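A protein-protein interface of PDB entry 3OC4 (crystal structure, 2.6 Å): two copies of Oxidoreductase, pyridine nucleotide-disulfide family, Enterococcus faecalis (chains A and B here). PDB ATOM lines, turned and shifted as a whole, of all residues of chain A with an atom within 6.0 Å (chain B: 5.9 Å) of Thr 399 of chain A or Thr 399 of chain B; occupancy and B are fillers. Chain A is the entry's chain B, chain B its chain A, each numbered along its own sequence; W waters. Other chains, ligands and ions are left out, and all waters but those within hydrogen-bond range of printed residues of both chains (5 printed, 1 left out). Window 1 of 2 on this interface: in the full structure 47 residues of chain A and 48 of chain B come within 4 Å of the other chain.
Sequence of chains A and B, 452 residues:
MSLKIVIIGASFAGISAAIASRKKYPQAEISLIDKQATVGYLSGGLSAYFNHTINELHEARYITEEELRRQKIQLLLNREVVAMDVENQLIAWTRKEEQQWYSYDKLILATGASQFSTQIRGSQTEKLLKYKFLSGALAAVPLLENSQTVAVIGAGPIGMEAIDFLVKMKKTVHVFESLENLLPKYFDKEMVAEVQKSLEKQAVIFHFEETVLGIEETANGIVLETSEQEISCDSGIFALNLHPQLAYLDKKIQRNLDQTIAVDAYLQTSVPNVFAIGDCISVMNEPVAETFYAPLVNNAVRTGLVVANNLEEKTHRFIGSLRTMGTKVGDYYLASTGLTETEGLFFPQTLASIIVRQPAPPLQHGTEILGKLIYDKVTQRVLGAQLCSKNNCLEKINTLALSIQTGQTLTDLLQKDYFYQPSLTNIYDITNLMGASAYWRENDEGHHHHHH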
ATOM      1  N   GLU A 395      16.839  13.879  20.579  1.00  0.00           N
ATOM      2  CA  GLU A 395      16.135  13.385  19.406  1.00  0.00           C
ATOM      3  C   GLU A 395      17.097  13.174  18.235  1.00  0.00           C
ATOM      4  O   GLU A 395      16.895  12.291  17.407  1.00  0.00           O
ATOM      5  CB  GLU A 395      15.026  14.363  19.012  1.00  0.00           C
ATOM      6  CG  GLU A 395      14.087  13.848  17.927  1.00  0.00           C
ATOM      7  CD  GLU A 395      13.289  12.614  18.355  1.00  0.00           C
ATOM      8  OE1 GLU A 395      12.731  12.609  19.486  1.00  0.00           O
ATOM      9  OE2 GLU A 395      13.206  11.657  17.548  1.00  0.00           O
ATOM     10  N   LYS A 396      18.154  13.978  18.174  1.00  0.00           N
ATOM     11  CA  LYS A 396      19.136  13.852  17.100  1.00  0.00           C
ATOM     12  C   LYS A 396      19.810  12.491  17.095  1.00  0.00           C
ATOM     13  O   LYS A 396      20.365  12.080  16.076  1.00  0.00           O
ATOM     14  CB  LYS A 396      20.192  14.962  17.189  1.00  0.00           C
ATOM     15  CG  LYS A 396      19.654  16.328  16.815  1.00  0.00           C
ATOM     16  CD  LYS A 396      20.748  17.378  16.773  1.00  0.00           C
ATOM     17  CE  LYS A 396      20.224  18.708  16.260  1.00  0.00           C
ATOM     18  NZ  LYS A 396      19.735  18.634  14.851  1.00  0.00           N
ATOM     19  N   ILE A 397      19.756  11.780  18.221  1.00  0.00           N
ATOM     20  CA  ILE A 397      20.370  10.462  18.265  1.00  0.00           C
ATOM     21  C   ILE A 397      19.490   9.471  17.503  1.00  0.00           C
ATOM     22  O   ILE A 397      19.998   8.522  16.909  1.00  0.00           O
ATOM     23  CB  ILE A 397      20.610   9.967  19.715  1.00  0.00           C
ATOM     24  CG1 ILE A 397      21.713   8.910  19.705  1.00  0.00           C
ATOM     25  CG2 ILE A 397      19.337   9.388  20.323  1.00  0.00           C
ATOM     26  CD1 ILE A 397      23.086   9.476  19.519  1.00  0.00           C
ATOM     27  N   ASN A 398      18.179   9.688  17.493  1.00  0.00           N
ATOM     28  CA  ASN A 398      17.314   8.763  16.751  1.00  0.00           C
ATOM     29  C   ASN A 398      17.620   8.875  15.261  1.00  0.00           C
ATOM     30  O   ASN A 398      17.596   7.874  14.531  1.00  0.00           O
ATOM     31  CB  ASN A 398      15.821   9.049  16.990  1.00  0.00           C
ATOM     32  CG  ASN A 398      15.383   8.716  18.399  1.00  0.00           C
ATOM     33  OD1 ASN A 398      15.822   7.730  18.982  1.00  0.00           O
ATOM     34  ND2 ASN A 398      14.502   9.535  18.950  1.00  0.00           N
ATOM     35  N   THR A 399      17.903  10.106  14.826  1.00  0.00           N
ATOM     36  CA  THR A 399      18.235  10.379  13.439  1.00  0.00           C
ATOM     37  C   THR A 399      19.599   9.750  13.131  1.00  0.00           C
ATOM     38  O   THR A 399      19.758   9.053  12.127  1.00  0.00           O
ATOM     39  CB  THR A 399      18.243  11.906  13.179  1.00  0.00           C
ATOM     40  OG1 THR A 399      16.959  12.443  13.540  1.00  0.00           O
ATOM     41  CG2 THR A 399      18.524  12.217  11.699  1.00  0.00           C
ATOM     42  N   LEU A 400      20.585   9.966  13.993  1.00  0.00           N
ATOM     43  CA  LEU A 400      21.888   9.353  13.749  1.00  0.00           C
ATOM     44  C   LEU A 400      21.793   7.824  13.737  1.00  0.00           C
ATOM     45  O   LEU A 400      22.514   7.160  12.990  1.00  0.00           O
ATOM     46  CB  LEU A 400      22.889   9.797  14.808  1.00  0.00           C
ATOM     47  CG  LEU A 400      23.405  11.218  14.564  1.00  0.00           C
ATOM     48  CD1 LEU A 400      23.911  11.769  15.855  1.00  0.00           C
ATOM     49  CD2 LEU A 400      24.487  11.220  13.487  1.00  0.00           C
ATOM     50  N   ALA A 401      20.905   7.270  14.565  1.00  0.00           N
ATOM     51  CA  ALA A 401      20.723   5.824  14.636  1.00  0.00           C
ATOM     52  C   ALA A 401      20.164   5.315  13.324  1.00  0.00           C
ATOM     53  O   ALA A 401      20.560   4.248  12.852  1.00  0.00           O
ATOM     54  CB  ALA A 401      19.778   5.449  15.786  1.00  0.00           C
ATOM     55  N   LEU A 402      19.241   6.078  12.740  1.00  0.00           N
ATOM     56  CA  LEU A 402      18.624   5.708  11.464  1.00  0.00           C
ATOM     57  C   LEU A 402      19.670   5.760  10.364  1.00  0.00           C
ATOM     58  O   LEU A 402      19.654   4.953   9.447  1.00  0.00           O
ATOM     59  CB  LEU A 402      17.469   6.644  11.127  1.00  0.00           C
ATOM     60  CG  LEU A 402      16.607   6.283   9.910  1.00  0.00           C
ATOM     61  CD1 LEU A 402      16.128   4.842  10.002  1.00  0.00           C
ATOM     62  CD2 LEU A 402      15.418   7.233   9.836  1.00  0.00           C
ATOM     63  N   SER A 403      20.602   6.699  10.476  1.00  0.00           N
ATOM     64  CA  SER A 403      21.667   6.813   9.492  1.00  0.00           C
ATOM     65  C   SER A 403      22.530   5.540   9.509  1.00  0.00           C
ATOM     66  O   SER A 403      22.796   4.935   8.468  1.00  0.00           O
ATOM     67  CB  SER A 403      22.527   8.034   9.799  1.00  0.00           C
ATOM     68  OG  SER A 403      23.556   8.176   8.842  1.00  0.00           O
ATOM     69  N   ILE A 404      22.963   5.135  10.698  1.00  0.00           N
ATOM     70  CA  ILE A 404      23.774   3.933  10.827  1.00  0.00           C
ATOM     71  C   ILE A 404      23.004   2.686  10.388  1.00  0.00           C
ATOM     72  O   ILE A 404      23.449   1.928   9.526  1.00  0.00           O
ATOM     73  CB  ILE A 404      24.228   3.722  12.293  1.00  0.00           C
ATOM     74  CG1 ILE A 404      25.109   4.885  12.749  1.00  0.00           C
ATOM     75  CG2 ILE A 404      24.977   2.404  12.422  1.00  0.00           C
ATOM     76  CD1 ILE A 404      25.215   4.993  14.251  1.00  0.00           C
ATOM     77  N   LYS A 416      22.236  14.593   3.861  1.00  0.00           N
ATOM     78  CA  LYS A 416      20.845  14.199   4.079  1.00  0.00           C
ATOM     79  C   LYS A 416      19.989  15.460   4.286  1.00  0.00           C
ATOM     80  O   LYS A 416      20.497  16.508   4.692  1.00  0.00           O
ATOM     81  CB  LYS A 416      20.715  13.290   5.307  1.00  0.00           C
ATOM     82  CG  LYS A 416      20.981  14.001   6.619  1.00  0.00           C
ATOM     83  CD  LYS A 416      21.011  13.050   7.811  1.00  0.00           C
ATOM     84  CE  LYS A 416      21.289  13.799   9.108  1.00  0.00           C
ATOM     85  NZ  LYS A 416      20.209  14.782   9.432  1.00  0.00           N
ATOM     86  N   THR A 431      24.162  17.007  12.907  1.00  0.00           N
ATOM     87  CA  THR A 431      24.209  15.596  12.499  1.00  0.00           C
ATOM     88  C   THR A 431      24.910  15.496  11.145  1.00  0.00           C
ATOM     89  O   THR A 431      25.840  14.713  10.972  1.00  0.00           O
ATOM     90  CB  THR A 431      22.792  14.946  12.436  1.00  0.00           C
ATOM     91  OG1 THR A 431      21.928  15.702  11.577  1.00  0.00           O
ATOM     92  CG2 THR A 431      22.196  14.869  13.840  1.00  0.00           C
ATOM     93  N   GLU B 395      12.402  18.119  15.474  1.00  0.00           N
ATOM     94  CA  GLU B 395      13.563  17.312  15.109  1.00  0.00           C
ATOM     95  C   GLU B 395      13.138  15.956  14.562  1.00  0.00           C
ATOM     96  O   GLU B 395      13.868  15.324  13.806  1.00  0.00           O
ATOM     97  CB  GLU B 395      14.499  17.131  16.317  1.00  0.00           C
ATOM     98  CG  GLU B 395      15.783  16.324  16.033  1.00  0.00           C
ATOM     99  CD  GLU B 395      16.776  17.016  15.062  1.00  0.00           C
ATOM    100  OE1 GLU B 395      17.014  18.248  15.198  1.00  0.00           O
ATOM    101  OE2 GLU B 395      17.336  16.308  14.180  1.00  0.00           O
ATOM    102  N   LYS B 396      11.947  15.509  14.943  1.00  0.00           N
ATOM    103  CA  LYS B 396      11.471  14.229  14.457  1.00  0.00           C
ATOM    104  C   LYS B 396      11.273  14.238  12.953  1.00  0.00           C
ATOM    105  O   LYS B 396      11.289  13.179  12.335  1.00  0.00           O
ATOM    106  CB  LYS B 396      10.178  13.825  15.176  1.00  0.00           C
ATOM    107  CG  LYS B 396      10.417  13.370  16.618  1.00  0.00           C
ATOM    108  CD  LYS B 396       9.156  12.839  17.281  1.00  0.00           C
ATOM    109  CE  LYS B 396       9.436  12.399  18.713  1.00  0.00           C
ATOM    110  NZ  LYS B 396      10.508  11.346  18.812  1.00  0.00           N
ATOM    111  N   ILE B 397      11.112  15.431  12.370  1.00  0.00           N
ATOM    112  CA  ILE B 397      10.919  15.572  10.925  1.00  0.00           C
ATOM    113  C   ILE B 397      12.219  15.200  10.212  1.00  0.00           C
ATOM    114  O   ILE B 397      12.211  14.708   9.081  1.00  0.00           O
ATOM    115  CB  ILE B 397      10.511  17.028  10.535  1.00  0.00           C
ATOM    116  CG1 ILE B 397       9.699  17.017   9.242  1.00  0.00           C
ATOM    117  CG2 ILE B 397      11.750  17.910  10.315  1.00  0.00           C
ATOM    118  CD1 ILE B 397       8.350  16.381   9.368  1.00  0.00           C
ATOM    119  N   ASN B 398      13.345  15.432  10.874  1.00  0.00           N
ATOM    120  CA  ASN B 398      14.626  15.081  10.269  1.00  0.00           C
ATOM    121  C   ASN B 398      14.791  13.569  10.221  1.00  0.00           C
ATOM    122  O   ASN B 398      15.490  13.036   9.352  1.00  0.00           O
ATOM    123  CB  ASN B 398      15.785  15.706  11.035  1.00  0.00           C
ATOM    124  CG  ASN B 398      15.799  17.213  10.919  1.00  0.00           C
ATOM    125  OD1 ASN B 398      15.516  17.769   9.853  1.00  0.00           O
ATOM    126  ND2 ASN B 398      16.144  17.888  12.009  1.00  0.00           N
ATOM    127  N   THR B 399      14.139  12.887  11.160  1.00  0.00           N
ATOM    128  CA  THR B 399      14.189  11.436  11.230  1.00  0.00           C
ATOM    129  C   THR B 399      13.257  10.912  10.135  1.00  0.00           C
ATOM    130  O   THR B 399      13.641  10.071   9.328  1.00  0.00           O
ATOM    131  CB  THR B 399      13.728  10.916  12.631  1.00  0.00           C
ATOM    132  OG1 THR B 399      14.523  11.533  13.658  1.00  0.00           O
ATOM    133  CG2 THR B 399      13.886   9.391  12.729  1.00  0.00           C
ATOM    134  N   LEU B 400      12.035  11.422  10.099  1.00  0.00           N
ATOM    135  CA  LEU B 400      11.088  11.008   9.079  1.00  0.00           C
ATOM    136  C   LEU B 400      11.627  11.285   7.673  1.00  0.00           C
ATOM    137  O   LEU B 400      11.400  10.504   6.749  1.00  0.00           O
ATOM    138  CB  LEU B 400       9.770  11.727   9.306  1.00  0.00           C
ATOM    139  CG  LEU B 400       9.078  11.124  10.528  1.00  0.00           C
ATOM    140  CD1 LEU B 400       8.036  12.072  11.049  1.00  0.00           C
ATOM    141  CD2 LEU B 400       8.484   9.755  10.159  1.00  0.00           C
ATOM    142  N   ALA B 401      12.353  12.390   7.519  1.00  0.00           N
ATOM    143  CA  ALA B 401      12.940  12.752   6.231  1.00  0.00           C
ATOM    144  C   ALA B 401      13.971  11.692   5.827  1.00  0.00           C
ATOM    145  O   ALA B 401      13.996  11.223   4.674  1.00  0.00           O
ATOM    146  CB  ALA B 401      13.607  14.123   6.325  1.00  0.00           C
ATOM    147  N   LEU B 402      14.825  11.330   6.780  1.00  0.00           N
ATOM    148  CA  LEU B 402      15.847  10.315   6.547  1.00  0.00           C
ATOM    149  C   LEU B 402      15.187   8.982   6.177  1.00  0.00           C
ATOM    150  O   LEU B 402      15.679   8.253   5.317  1.00  0.00           O
ATOM    151  CB  LEU B 402      16.691  10.104   7.800  1.00  0.00           C
ATOM    152  CG  LEU B 402      18.213  10.002   7.659  1.00  0.00           C
ATOM    153  CD1 LEU B 402      18.746   9.357   8.929  1.00  0.00           C
ATOM    154  CD2 LEU B 402      18.630   9.205   6.426  1.00  0.00           C
ATOM    155  N   SER B 403      14.072   8.668   6.828  1.00  0.00           N
ATOM    156  CA  SER B 403      13.363   7.419   6.573  1.00  0.00           C
ATOM    157  C   SER B 403      12.924   7.322   5.098  1.00  0.00           C
ATOM    158  O   SER B 403      13.113   6.286   4.447  1.00  0.00           O
ATOM    159  CB  SER B 403      12.155   7.312   7.516  1.00  0.00           C
ATOM    160  OG  SER B 403      11.520   6.045   7.433  1.00  0.00           O
ATOM    161  N   ILE B 404      12.356   8.410   4.578  1.00  0.00           N
ATOM    162  CA  ILE B 404      11.903   8.471   3.187  1.00  0.00           C
ATOM    163  C   ILE B 404      13.084   8.462   2.198  1.00  0.00           C
ATOM    164  O   ILE B 404      13.073   7.778   1.172  1.00  0.00           O
ATOM    165  CB  ILE B 404      11.084   9.760   2.949  1.00  0.00           C
ATOM    166  CG1 ILE B 404       9.873   9.791   3.882  1.00  0.00           C
ATOM    167  CG2 ILE B 404      10.663   9.851   1.495  1.00  0.00           C
ATOM    168  CD1 ILE B 404       9.188  11.135   3.947  1.00  0.00           C
ATOM    169  N   LYS B 416      12.560   0.644  13.417  1.00  0.00           N
ATOM    170  CA  LYS B 416      13.868   1.301  13.458  1.00  0.00           C
ATOM    171  C   LYS B 416      14.243   1.579  14.914  1.00  0.00           C
ATOM    172  O   LYS B 416      13.377   1.711  15.770  1.00  0.00           O
ATOM    173  CB  LYS B 416      13.834   2.630  12.698  1.00  0.00           C
ATOM    174  CG  LYS B 416      12.980   3.707  13.376  1.00  0.00           C
ATOM    175  CD  LYS B 416      12.934   4.983  12.570  1.00  0.00           C
ATOM    176  CE  LYS B 416      12.141   6.066  13.286  1.00  0.00           C
ATOM    177  NZ  LYS B 416      12.809   6.443  14.558  1.00  0.00           N
ATOM    178  N   THR B 431       7.288   8.336  15.791  1.00  0.00           N
ATOM    179  CA  THR B 431       7.764   8.156  14.420  1.00  0.00           C
ATOM    180  C   THR B 431       7.600   6.702  13.993  1.00  0.00           C
ATOM    181  O   THR B 431       7.144   6.418  12.889  1.00  0.00           O
ATOM    182  CB  THR B 431       9.246   8.592  14.252  1.00  0.00           C
ATOM    183  OG1 THR B 431      10.112   7.671  14.921  1.00  0.00           O
ATOM    184  CG2 THR B 431       9.449   9.970  14.829  1.00  0.00           C
HETATM  185  O   HOH W   1      11.068  10.868  21.626  1.00  0.00           O
HETATM  186  O   HOH W   2      19.000  16.157  11.770  1.00  0.00           O
HETATM  187  O   HOH W   3      18.009  21.171  14.473  1.00  0.00           O
HETATM  188  O   HOH W   4      12.512   8.621  16.086  1.00  0.00           O
HETATM  189  O   HOH W   5      17.743  14.171   8.415  1.00  0.00           O
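NZ of Lys 396 of chain A lies within salt-bridge range of OE1 of Glu 395 of chain B, at 2.8 Å. The side-chain amino group (NZ) of Lys 396 of chain B lies within salt-bridge range of the side-chain carboxylate (OE1) of Glu 395 of chain A (2.6 Å). The side-chain hydroxyl (OG1) of Thr 399 of chain B sits at hydrogen-bond distance from the side-chain hydroxyl (OG1) of Thr 399 of chain A (2.6 Å).
The side-chain carboxylate of Glu 395 of chain B lies within hydrogen-bond range of the side-chain amide nitrogen of Asn 398 of chain B, 2.9 Å away. The side-chain carboxylate (OE2) of Glu 395 of chain A is in hydrogen-bond range of the side-chain amide nitrogen (ND2) of Asn 398 of chain A, at 2.9 Å.
Glu 395 of chain A touches Glu 395 of chain B (CG to CG, 3.5 Å). OE2 of Glu 395 of chain B touches OG1 of Thr 399 of chain A, 3.9 Å away. Thr 399 of chain A touches Asn 398 of chain B (CG2 to O, 3.9 Å). O of Thr 399 of chain A touches CD1 of Leu 402 of chain B (3.4 Å). Leu 402 of chain A touches Thr 399 of chain B. Leu 402 of chain A touches Leu 402 of chain B. CD2 of Leu 402 of chain A touches N of Ser 403 of chain B, at 3.6 Å. CD1 of Leu 402 of chain B touches N of Ser 403 of chain A, at 3.6 Å.
Of chain B, only Glu 395, Asn 398, Thr 399 and Leu 402 come within 4 Å of Thr 399 of chain A. Printed residues of chain B within 4 Å of Ser 403 of chain A: Leu 402 (3.6 Å). Of the printed residues of chain A, Glu 395 of chain B touches Glu 395 (3.5 Å), Lys 396 (2.8 Å) and Thr 399 (3.9 Å). Ile 397 of chain B touches none of the printed residues of chain A. Thr 399 of chain B touches just these residues of chain A: Thr 399 and Leu 402. Printed residues of chain A within 4 Å of Ser 403 of chain B: Leu 402 (3.6 Å). The nearest residue of chain B that does not touch Thr 399 of chain A is Lys 396 of chain B (5.8 Å). The nearest residue of chain A that does not touch Thr 399 of chain B is Glu 395 of chain A (4.1 Å).
Hydrophobic or aromatic side chains of chain A that line the printed part of chain B: Leu 402. Of the 12 printed residues of chain B, 6 touch a printed residue of chain A. Printed residues of chain B that touch a printed residue of chain A: Glu 395, Lys 396, Asn 398, Thr 399, Leu 402 and Ser 403. Among the printed residues, Asp or Glu carboxylates within 4 Å of a Lys or Arg side-chain nitrogen of the other chain: Glu 395 of chain A with Lys 396 of chain B (2.6 Å) and Lys 396 of chain A with Glu 395 of chain B (2.8 Å).
Thr 399 of chain B touches its own counterpart, Thr 399 of chain A. Thr 399 of chain A touches Leu 402 of chain B, and with the chains exchanged Leu 402 of chain A touches Thr 399 of chain B. Leu 402 of chain B touches its own counterpart, Leu 402 of chain A. Leu 402 of chain A touches Ser 403 of chain B, and with the chains exchanged Ser 403 of chain A touches Leu 402 of chain B. Positions printed for both chains: 395, 396, 397, 398, 399, 400, 401, 402, 403, 404, 416 and 431.
Water W4 lies within hydrogen-bond range of NZ of Lys 416 of chain B (2.7 Å), OG1 of Thr 431 of chain B (2.8 Å) and OE2 of Glu 395 of chain A (3.4 Å). Water W5 lies within hydrogen-bond range of the backbone carbonyl oxygen of Asn 398 of chain B (2.7 Å) and the side-chain amino group of Lys 416 of chain A (2.7 Å). Water W1 bridges NZ of Lys 396 of chain B (2.9 Å) and OE1 of Glu 395 of chain A (3.2 Å). Water W2 lies within hydrogen-bond range of OE2 of Glu 395 of chain B (2.9 Å), OG1 of Thr 431 of chain A (3.0 Å), NZ of Lys 416 of chain A (3.0 Å) and ND2 of Asn 398 of chain B (3.3 Å). Water W3 bridges NZ of Lys 396 of chain A (3.1 Å) and OE1 of Glu 395 of chain B (3.2 Å).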
